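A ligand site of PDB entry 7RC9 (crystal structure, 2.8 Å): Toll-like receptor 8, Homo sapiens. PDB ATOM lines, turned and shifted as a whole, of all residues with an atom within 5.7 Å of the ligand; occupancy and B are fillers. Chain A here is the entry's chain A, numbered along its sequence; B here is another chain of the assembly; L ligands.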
ATOM      1  N   PHE A 239     -30.380   7.330  -0.106  1.00  0.00           N
ATOM      2  CA  PHE A 239     -30.160   7.432   1.328  1.00  0.00           C
ATOM      3  C   PHE A 239     -29.881   6.048   1.924  1.00  0.00           C
ATOM      4  O   PHE A 239     -29.296   5.197   1.243  1.00  0.00           O
ATOM      5  CB  PHE A 239     -31.402   8.060   1.967  1.00  0.00           C
ATOM      6  CG  PHE A 239     -31.100   9.271   2.817  1.00  0.00           C
ATOM      7  CD1 PHE A 239     -31.135  10.548   2.273  1.00  0.00           C
ATOM      8  CD2 PHE A 239     -30.786   9.132   4.172  1.00  0.00           C
ATOM      9  CE1 PHE A 239     -30.853  11.665   3.062  1.00  0.00           C
ATOM     10  CE2 PHE A 239     -30.511  10.250   4.954  1.00  0.00           C
ATOM     11  CZ  PHE A 239     -30.552  11.498   4.394  1.00  0.00           C
ATOM     12  N   PHE A 324     -36.150  14.905   5.427  1.00  0.00           N
ATOM     13  CA  PHE A 324     -34.909  14.724   4.667  1.00  0.00           C
ATOM     14  C   PHE A 324     -34.917  15.463   3.320  1.00  0.00           C
ATOM     15  O   PHE A 324     -34.680  14.872   2.266  1.00  0.00           O
ATOM     16  CB  PHE A 324     -34.548  13.227   4.545  1.00  0.00           C
ATOM     17  CG  PHE A 324     -34.374  12.584   5.901  1.00  0.00           C
ATOM     18  CD1 PHE A 324     -33.197  12.760   6.629  1.00  0.00           C
ATOM     19  CD2 PHE A 324     -35.396  11.836   6.468  1.00  0.00           C
ATOM     20  CE1 PHE A 324     -33.048  12.190   7.889  1.00  0.00           C
ATOM     21  CE2 PHE A 324     -35.241  11.264   7.735  1.00  0.00           C
ATOM     22  CZ  PHE A 324     -34.070  11.442   8.442  1.00  0.00           C
ATOM     23  N   TYR A 326     -33.210  18.539   3.213  1.00  0.00           N
ATOM     24  CA  TYR A 326     -32.017  19.341   3.447  1.00  0.00           C
ATOM     25  C   TYR A 326     -31.126  19.569   2.229  1.00  0.00           C
ATOM     26  O   TYR A 326     -31.045  18.715   1.350  1.00  0.00           O
ATOM     27  CB  TYR A 326     -31.164  18.736   4.598  1.00  0.00           C
ATOM     28  CG  TYR A 326     -30.412  17.483   4.228  1.00  0.00           C
ATOM     29  CD1 TYR A 326     -31.041  16.238   4.217  1.00  0.00           C
ATOM     30  CD2 TYR A 326     -29.049  17.530   3.901  1.00  0.00           C
ATOM     31  CE1 TYR A 326     -30.348  15.079   3.857  1.00  0.00           C
ATOM     32  CE2 TYR A 326     -28.356  16.371   3.555  1.00  0.00           C
ATOM     33  CZ  TYR A 326     -29.008  15.152   3.530  1.00  0.00           C
ATOM     34  OH  TYR A 326     -28.327  14.005   3.199  1.00  0.00           O
ATOM     35  N   ILE A 327     -30.420  20.706   2.224  1.00  0.00           N
ATOM     36  CA  ILE A 327     -29.431  21.035   1.205  1.00  0.00           C
ATOM     37  C   ILE A 327     -28.106  20.490   1.763  1.00  0.00           C
ATOM     38  O   ILE A 327     -27.771  20.755   2.925  1.00  0.00           O
ATOM     39  CB  ILE A 327     -29.381  22.550   0.837  1.00  0.00           C
ATOM     40  CG1 ILE A 327     -30.756  23.071   0.348  1.00  0.00           C
ATOM     41  CG2 ILE A 327     -28.269  22.842  -0.194  1.00  0.00           C
ATOM     42  CD1 ILE A 327     -30.922  24.618   0.287  1.00  0.00           C
ATOM     43  N   LYS A 328     -27.396  19.700   0.953  1.00  0.00           N
ATOM     44  CA  LYS A 328     -26.101  19.092   1.274  1.00  0.00           C
ATOM     45  C   LYS A 328     -25.067  20.194   1.538  1.00  0.00           C
ATOM     46  O   LYS A 328     -24.877  21.088   0.699  1.00  0.00           O
ATOM     47  CB  LYS A 328     -25.664  18.186   0.104  1.00  0.00           C
ATOM     48  CG  LYS A 328     -24.665  17.096   0.493  1.00  0.00           C
ATOM     49  CD  LYS A 328     -24.075  16.385  -0.727  1.00  0.00           C
ATOM     50  CE  LYS A 328     -22.821  17.041  -1.270  1.00  0.00           C
ATOM     51  NZ  LYS A 328     -22.316  16.369  -2.484  1.00  0.00           N
ATOM     52  N   GLY A 329     -24.461  20.153   2.729  1.00  0.00           N
ATOM     53  CA  GLY A 329     -23.448  21.107   3.170  1.00  0.00           C
ATOM     54  C   GLY A 329     -24.016  22.390   3.751  1.00  0.00           C
ATOM     55  O   GLY A 329     -23.258  23.269   4.160  1.00  0.00           O
ATOM     56  N   SER A 330     -25.355  22.496   3.817  1.00  0.00           N
ATOM     57  CA  SER A 330     -26.046  23.676   4.333  1.00  0.00           C
ATOM     58  C   SER A 330     -26.633  23.465   5.730  1.00  0.00           C
ATOM     59  O   SER A 330     -27.531  22.657   5.930  1.00  0.00           O
ATOM     60  CB  SER A 330     -27.111  24.155   3.348  1.00  0.00           C
ATOM     61  OG  SER A 330     -27.510  25.490   3.618  1.00  0.00           O
ATOM     62  N   TYR A 331     -26.093  24.218   6.701  1.00  0.00           N
ATOM     63  CA  TYR A 331     -26.501  24.224   8.099  1.00  0.00           C
ATOM     64  C   TYR A 331     -27.025  25.654   8.426  1.00  0.00           C
ATOM     65  O   TYR A 331     -26.295  26.457   9.022  1.00  0.00           O
ATOM     66  CB  TYR A 331     -25.297  23.812   8.985  1.00  0.00           C
ATOM     67  CG  TYR A 331     -25.613  23.386  10.408  1.00  0.00           C
ATOM     68  CD1 TYR A 331     -26.881  22.948  10.770  1.00  0.00           C
ATOM     69  CD2 TYR A 331     -24.621  23.364  11.384  1.00  0.00           C
ATOM     70  CE1 TYR A 331     -27.165  22.522  12.066  1.00  0.00           C
ATOM     71  CE2 TYR A 331     -24.887  22.954  12.682  1.00  0.00           C
ATOM     72  CZ  TYR A 331     -26.160  22.528  13.023  1.00  0.00           C
ATOM     73  OH  TYR A 331     -26.437  22.102  14.298  1.00  0.00           O
ATOM     74  N   GLY A 354     -34.798  15.935   9.273  1.00  0.00           N
ATOM     75  CA  GLY A 354     -33.702  16.134   8.329  1.00  0.00           C
ATOM     76  C   GLY A 354     -33.753  17.340   7.420  1.00  0.00           C
ATOM     77  O   GLY A 354     -33.392  17.241   6.250  1.00  0.00           O
ATOM     78  N   VAL A 356     -32.377  20.117   8.727  1.00  0.00           N
ATOM     79  CA  VAL A 356     -31.072  20.531   9.272  1.00  0.00           C
ATOM     80  C   VAL A 356     -30.993  22.053   9.422  1.00  0.00           C
ATOM     81  O   VAL A 356     -30.860  22.773   8.440  1.00  0.00           O
ATOM     82  CB  VAL A 356     -29.836  19.930   8.536  1.00  0.00           C
ATOM     83  CG1 VAL A 356     -28.552  20.171   9.320  1.00  0.00           C
ATOM     84  CG2 VAL A 356     -30.016  18.435   8.277  1.00  0.00           C
ATOM     85  N   ILE A 381     -33.879  14.463  14.160  1.00  0.00           N
ATOM     86  CA  ILE A 381     -32.687  14.474  13.273  1.00  0.00           C
ATOM     87  C   ILE A 381     -32.597  15.807  12.488  1.00  0.00           C
ATOM     88  O   ILE A 381     -32.630  15.817  11.255  1.00  0.00           O
ATOM     89  CB  ILE A 381     -32.589  13.198  12.367  1.00  0.00           C
ATOM     90  CG1 ILE A 381     -32.990  11.903  13.132  1.00  0.00           C
ATOM     91  CG2 ILE A 381     -31.188  13.066  11.764  1.00  0.00           C
ATOM     92  CD1 ILE A 381     -33.669  10.854  12.314  1.00  0.00           C
ATOM     93  N   PHE A 383     -30.529  18.433  14.183  1.00  0.00           N
ATOM     94  CA  PHE A 383     -29.331  18.934  14.863  1.00  0.00           C
ATOM     95  C   PHE A 383     -29.516  20.315  15.488  1.00  0.00           C
ATOM     96  O   PHE A 383     -28.536  21.059  15.600  1.00  0.00           O
ATOM     97  CB  PHE A 383     -28.111  18.901  13.912  1.00  0.00           C
ATOM     98  CG  PHE A 383     -27.819  17.546  13.319  1.00  0.00           C
ATOM     99  CD1 PHE A 383     -26.987  16.642  13.981  1.00  0.00           C
ATOM    100  CD2 PHE A 383     -28.352  17.163  12.090  1.00  0.00           C
ATOM    101  CE1 PHE A 383     -26.710  15.391  13.428  1.00  0.00           C
ATOM    102  CE2 PHE A 383     -28.074  15.912  11.537  1.00  0.00           C
ATOM    103  CZ  PHE A 383     -27.250  15.040  12.214  1.00  0.00           C
ATOM    104  N   GLU A 405     -33.029  13.075  18.701  1.00  0.00           N
ATOM    105  CA  GLU A 405     -31.814  13.098  17.880  1.00  0.00           C
ATOM    106  C   GLU A 405     -31.417  14.532  17.419  1.00  0.00           C
ATOM    107  O   GLU A 405     -31.009  14.748  16.272  1.00  0.00           O
ATOM    108  CB  GLU A 405     -31.891  12.090  16.705  1.00  0.00           C
ATOM    109  CG  GLU A 405     -31.740  10.640  17.138  1.00  0.00           C
ATOM    110  CD  GLU A 405     -32.360   9.593  16.237  1.00  0.00           C
ATOM    111  OE1 GLU A 405     -31.709   8.550  16.016  1.00  0.00           O
ATOM    112  OE2 GLU A 405     -33.518   9.788  15.795  1.00  0.00           O
ATOM    113  N   PHE B 472     -21.001  16.678  12.134  1.00  0.00           N
ATOM    114  CA  PHE B 472     -21.818  15.762  11.325  1.00  0.00           C
ATOM    115  C   PHE B 472     -21.558  15.897   9.809  1.00  0.00           C
ATOM    116  O   PHE B 472     -22.067  15.096   9.021  1.00  0.00           O
ATOM    117  CB  PHE B 472     -23.308  15.864  11.684  1.00  0.00           C
ATOM    118  CG  PHE B 472     -23.965  17.208  11.487  1.00  0.00           C
ATOM    119  CD1 PHE B 472     -23.995  18.144  12.521  1.00  0.00           C
ATOM    120  CD2 PHE B 472     -24.637  17.509  10.313  1.00  0.00           C
ATOM    121  CE1 PHE B 472     -24.648  19.372  12.361  1.00  0.00           C
ATOM    122  CE2 PHE B 472     -25.284  18.735  10.146  1.00  0.00           C
ATOM    123  CZ  PHE B 472     -25.272  19.663  11.167  1.00  0.00           C
ATOM    124  N   PHE B 473     -20.744  16.897   9.418  1.00  0.00           N
ATOM    125  CA  PHE B 473     -20.230  17.183   8.079  1.00  0.00           C
ATOM    126  C   PHE B 473     -19.060  18.161   8.186  1.00  0.00           C
ATOM    127  O   PHE B 473     -19.024  18.965   9.123  1.00  0.00           O
ATOM    128  CB  PHE B 473     -21.316  17.658   7.072  1.00  0.00           C
ATOM    129  CG  PHE B 473     -21.745  19.102   7.133  1.00  0.00           C
ATOM    130  CD1 PHE B 473     -21.053  20.084   6.434  1.00  0.00           C
ATOM    131  CD2 PHE B 473     -22.900  19.473   7.819  1.00  0.00           C
ATOM    132  CE1 PHE B 473     -21.455  21.420   6.484  1.00  0.00           C
ATOM    133  CE2 PHE B 473     -23.318  20.803   7.854  1.00  0.00           C
ATOM    134  CZ  PHE B 473     -22.587  21.764   7.197  1.00  0.00           C
ATOM    135  N   SER B 494     -19.985  11.086  13.661  1.00  0.00           N
ATOM    136  CA  SER B 494     -21.154  10.772  12.806  1.00  0.00           C
ATOM    137  C   SER B 494     -21.086  11.633  11.545  1.00  0.00           C
ATOM    138  O   SER B 494     -22.096  12.175  11.095  1.00  0.00           O
ATOM    139  CB  SER B 494     -22.475  10.951  13.556  1.00  0.00           C
ATOM    140  OG  SER B 494     -22.678   9.911  14.494  1.00  0.00           O
ATOM    141  N   ASN B 495     -19.875  11.796  11.013  1.00  0.00           N
ATOM    142  CA  ASN B 495     -19.597  12.636   9.856  1.00  0.00           C
ATOM    143  C   ASN B 495     -20.073  11.977   8.573  1.00  0.00           C
ATOM    144  O   ASN B 495     -19.498  10.970   8.167  1.00  0.00           O
ATOM    145  CB  ASN B 495     -18.108  12.979   9.794  1.00  0.00           C
ATOM    146  CG  ASN B 495     -17.826  14.304   9.148  1.00  0.00           C
ATOM    147  OD1 ASN B 495     -18.087  14.505   7.967  1.00  0.00           O
ATOM    148  ND2 ASN B 495     -17.270  15.219   9.907  1.00  0.00           N
ATOM    149  N   ALA B 496     -21.122  12.557   7.961  1.00  0.00           N
ATOM    150  CA  ALA B 496     -21.752  12.093   6.718  1.00  0.00           C
ATOM    151  C   ALA B 496     -21.366  12.993   5.531  1.00  0.00           C
ATOM    152  O   ALA B 496     -22.199  13.313   4.679  1.00  0.00           O
ATOM    153  CB  ALA B 496     -23.266  12.037   6.878  1.00  0.00           C
ATOM    154  N   GLN B 497     -20.084  13.382   5.479  1.00  0.00           N
ATOM    155  CA  GLN B 497     -19.522  14.236   4.423  1.00  0.00           C
ATOM    156  C   GLN B 497     -19.255  13.467   3.127  1.00  0.00           C
ATOM    157  O   GLN B 497     -18.717  12.363   3.162  1.00  0.00           O
ATOM    158  CB  GLN B 497     -18.227  14.900   4.929  1.00  0.00           C
ATOM    159  CG  GLN B 497     -17.517  15.841   3.952  1.00  0.00           C
ATOM    160  CD  GLN B 497     -18.282  17.111   3.656  1.00  0.00           C
ATOM    161  OE1 GLN B 497     -18.834  17.769   4.549  1.00  0.00           O
ATOM    162  NE2 GLN B 497     -18.320  17.493   2.383  1.00  0.00           N
ATOM    163  N   VAL B 498     -19.606  14.084   1.998  1.00  0.00           N
ATOM    164  CA  VAL B 498     -19.314  13.526   0.678  1.00  0.00           C
ATOM    165  C   VAL B 498     -17.971  14.164   0.299  1.00  0.00           C
ATOM    166  O   VAL B 498     -17.923  15.341  -0.070  1.00  0.00           O
ATOM    167  CB  VAL B 498     -20.444  13.797  -0.354  1.00  0.00           C
ATOM    168  CG1 VAL B 498     -20.098  13.187  -1.711  1.00  0.00           C
ATOM    169  CG2 VAL B 498     -21.787  13.266   0.136  1.00  0.00           C
ATOM    170  N   ARG B 519     -19.837   8.270   8.890  1.00  0.00           N
ATOM    171  CA  ARG B 519     -20.760   7.903   7.820  1.00  0.00           C
ATOM    172  C   ARG B 519     -20.341   8.547   6.481  1.00  0.00           C
ATOM    173  O   ARG B 519     -21.179   8.917   5.660  1.00  0.00           O
ATOM    174  CB  ARG B 519     -22.198   8.279   8.214  1.00  0.00           C
ATOM    175  CG  ARG B 519     -22.788   7.437   9.341  1.00  0.00           C
ATOM    176  CD  ARG B 519     -24.174   7.916   9.714  1.00  0.00           C
ATOM    177  NE  ARG B 519     -24.926   6.894  10.445  1.00  0.00           N
ATOM    178  CZ  ARG B 519     -25.019   6.845  11.772  1.00  0.00           C
ATOM    179  NH1 ARG B 519     -25.740   5.886  12.352  1.00  0.00           N
ATOM    180  NH2 ARG B 519     -24.414   7.749  12.525  1.00  0.00           N
ATOM    181  N   TYR B 545     -23.953   6.019   4.095  1.00  0.00           N
ATOM    182  CA  TYR B 545     -25.301   6.528   4.328  1.00  0.00           C
ATOM    183  C   TYR B 545     -26.016   6.957   3.046  1.00  0.00           C
ATOM    184  O   TYR B 545     -27.218   7.219   3.066  1.00  0.00           O
ATOM    185  CB  TYR B 545     -25.228   7.699   5.340  1.00  0.00           C
ATOM    186  CG  TYR B 545     -26.434   7.823   6.260  1.00  0.00           C
ATOM    187  CD1 TYR B 545     -26.966   6.707   6.902  1.00  0.00           C
ATOM    188  CD2 TYR B 545     -26.993   9.058   6.542  1.00  0.00           C
ATOM    189  CE1 TYR B 545     -28.058   6.818   7.768  1.00  0.00           C
ATOM    190  CE2 TYR B 545     -28.080   9.189   7.410  1.00  0.00           C
ATOM    191  CZ  TYR B 545     -28.609   8.054   8.015  1.00  0.00           C
ATOM    192  OH  TYR B 545     -29.685   8.173   8.868  1.00  0.00           O
ATOM    193  N   PHE B 546     -25.279   7.018   1.915  1.00  0.00           N
ATOM    194  CA  PHE B 546     -25.812   7.449   0.617  1.00  0.00           C
ATOM    195  C   PHE B 546     -25.439   6.452  -0.502  1.00  0.00           C
ATOM    196  O   PHE B 546     -25.001   6.874  -1.582  1.00  0.00           O
ATOM    197  CB  PHE B 546     -25.345   8.891   0.300  1.00  0.00           C
ATOM    198  CG  PHE B 546     -25.335   9.852   1.471  1.00  0.00           C
ATOM    199  CD1 PHE B 546     -24.151  10.185   2.107  1.00  0.00           C
ATOM    200  CD2 PHE B 546     -26.521  10.395   1.951  1.00  0.00           C
ATOM    201  CE1 PHE B 546     -24.148  11.049   3.203  1.00  0.00           C
ATOM    202  CE2 PHE B 546     -26.525  11.260   3.053  1.00  0.00           C
ATOM    203  CZ  PHE B 546     -25.335  11.582   3.668  1.00  0.00           C
HETATM  204  C1  LIG L   1     -28.314  10.503  11.876  1.00  0.00           C
HETATM  205  C2  LIG L   1     -28.411  10.973  13.297  1.00  0.00           C
HETATM  206  C3  LIG L   1     -27.934   9.056  11.692  1.00  0.00           C
HETATM  207  C4  LIG L   1     -26.010  18.308   5.885  1.00  0.00           C
HETATM  208  C5  LIG L   1     -24.135  16.842   4.887  1.00  0.00           C
HETATM  209  C6  LIG L   1     -28.721  13.281   6.540  1.00  0.00           C
HETATM  210  C7  LIG L   1     -26.797  19.606   5.923  1.00  0.00           C
HETATM  211  C8  LIG L   1     -27.336  11.459  11.069  1.00  0.00           C
HETATM  212  C9  LIG L   1     -25.892  11.535  11.411  1.00  0.00           C
HETATM  213  C10 LIG L   1     -25.001  12.495  10.674  1.00  0.00           C
HETATM  214  C11 LIG L   1     -25.594  13.393   9.523  1.00  0.00           C
HETATM  215  C12 LIG L   1     -26.940  13.336   9.192  1.00  0.00           C
HETATM  216  C13 LIG L   1     -27.891  12.335   9.975  1.00  0.00           C
HETATM  217  N1  LIG L   1     -24.990  14.327   8.726  1.00  0.00           N
HETATM  218  C14 LIG L   1     -25.929  14.824   7.865  1.00  0.00           C
HETATM  219  C15 LIG L   1     -27.168  14.258   8.194  1.00  0.00           C
HETATM  220  C16 LIG L   1     -28.476  14.503   7.417  1.00  0.00           C
HETATM  221  C17 LIG L   1     -29.699  14.777   8.295  1.00  0.00           C
HETATM  222  C18 LIG L   1     -29.162  10.003  14.222  1.00  0.00           C
HETATM  223  N2  LIG L   1     -28.741   8.577  14.034  1.00  0.00           N
HETATM  224  C19 LIG L   1     -28.744   8.119  12.610  1.00  0.00           C
HETATM  225  C20 LIG L   1     -25.612  15.916   6.834  1.00  0.00           C
HETATM  226  C21 LIG L   1     -26.356  17.214   6.887  1.00  0.00           C
HETATM  227  N3  LIG L   1     -24.907  18.107   4.916  1.00  0.00           N
HETATM  228  C22 LIG L   1     -24.487  15.720   5.873  1.00  0.00           C
HETATM  229  C23 LIG L   1     -23.015  16.650   3.876  1.00  0.00           C
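The backbone carbonyl oxygen (O) of Phe 472 of chain B sits at hydrogen-bond distance from a nitrogen (N1) of the ligand, 3.0 Å away. N of Gly 329 is in hydrogen-bond range of N3 of the ligand, at 3.0 Å. A nitrogen (N2) of the ligand is in salt-bridge range of the side-chain carboxylate (OE1) of Glu 405, at 3.6 Å.
O of Phe 383 sits at hydrogen-bond distance from OH of Tyr 331 (2.7 Å). The backbone carbonyl oxygen (O) of Phe 472 of chain B lies within hydrogen-bond range of the backbone NH (N) of Ala 496 of chain B (2.9 Å). N of Gly 354 lies within hydrogen-bond range of O of Ile 381 (2.9 Å). The guanidinium group of Arg 519 of chain B lies within hydrogen-bond range of the side-chain hydroxyl of Ser 494 of chain B, 3.4 Å away. The backbone NH (N) of Tyr 326 lies close to the backbone carbonyl oxygen (O) of Gly 354.
Residues that only touch the ligand: Ser 494 of chain B (3.0 Å), Ser 330 (3.1 Å), Phe 239 (3.3 Å), Ile 327 (3.4 Å), Ala 496 of chain B (3.4 Å), Tyr 545 of chain B (3.4 Å), Tyr 326 (3.4 Å), Phe 383 (3.5 Å), Phe 473 of chain B (3.7 Å), Arg 519 of chain B (3.7 Å), Val 356 (3.7 Å), Lys 328 (3.8 Å) and Ile 381 (3.8 Å). Within 4 Å of the ligand: Phe 239, Tyr 326, Ile 327, Lys 328, Gly 329, Ser 330, Val 356, Ile 381, Phe 383, Glu 405, Phe 472 of chain B, Phe 473 of chain B, Ser 494 of chain B, Ala 496 of chain B, Arg 519 of chain B and Tyr 545 of chain B. Along chain A the residues within 4 Å of the ligand span positions 239 to 405. The nearest printed residue that does not touch the ligand is Gly 354 (4.2 Å).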
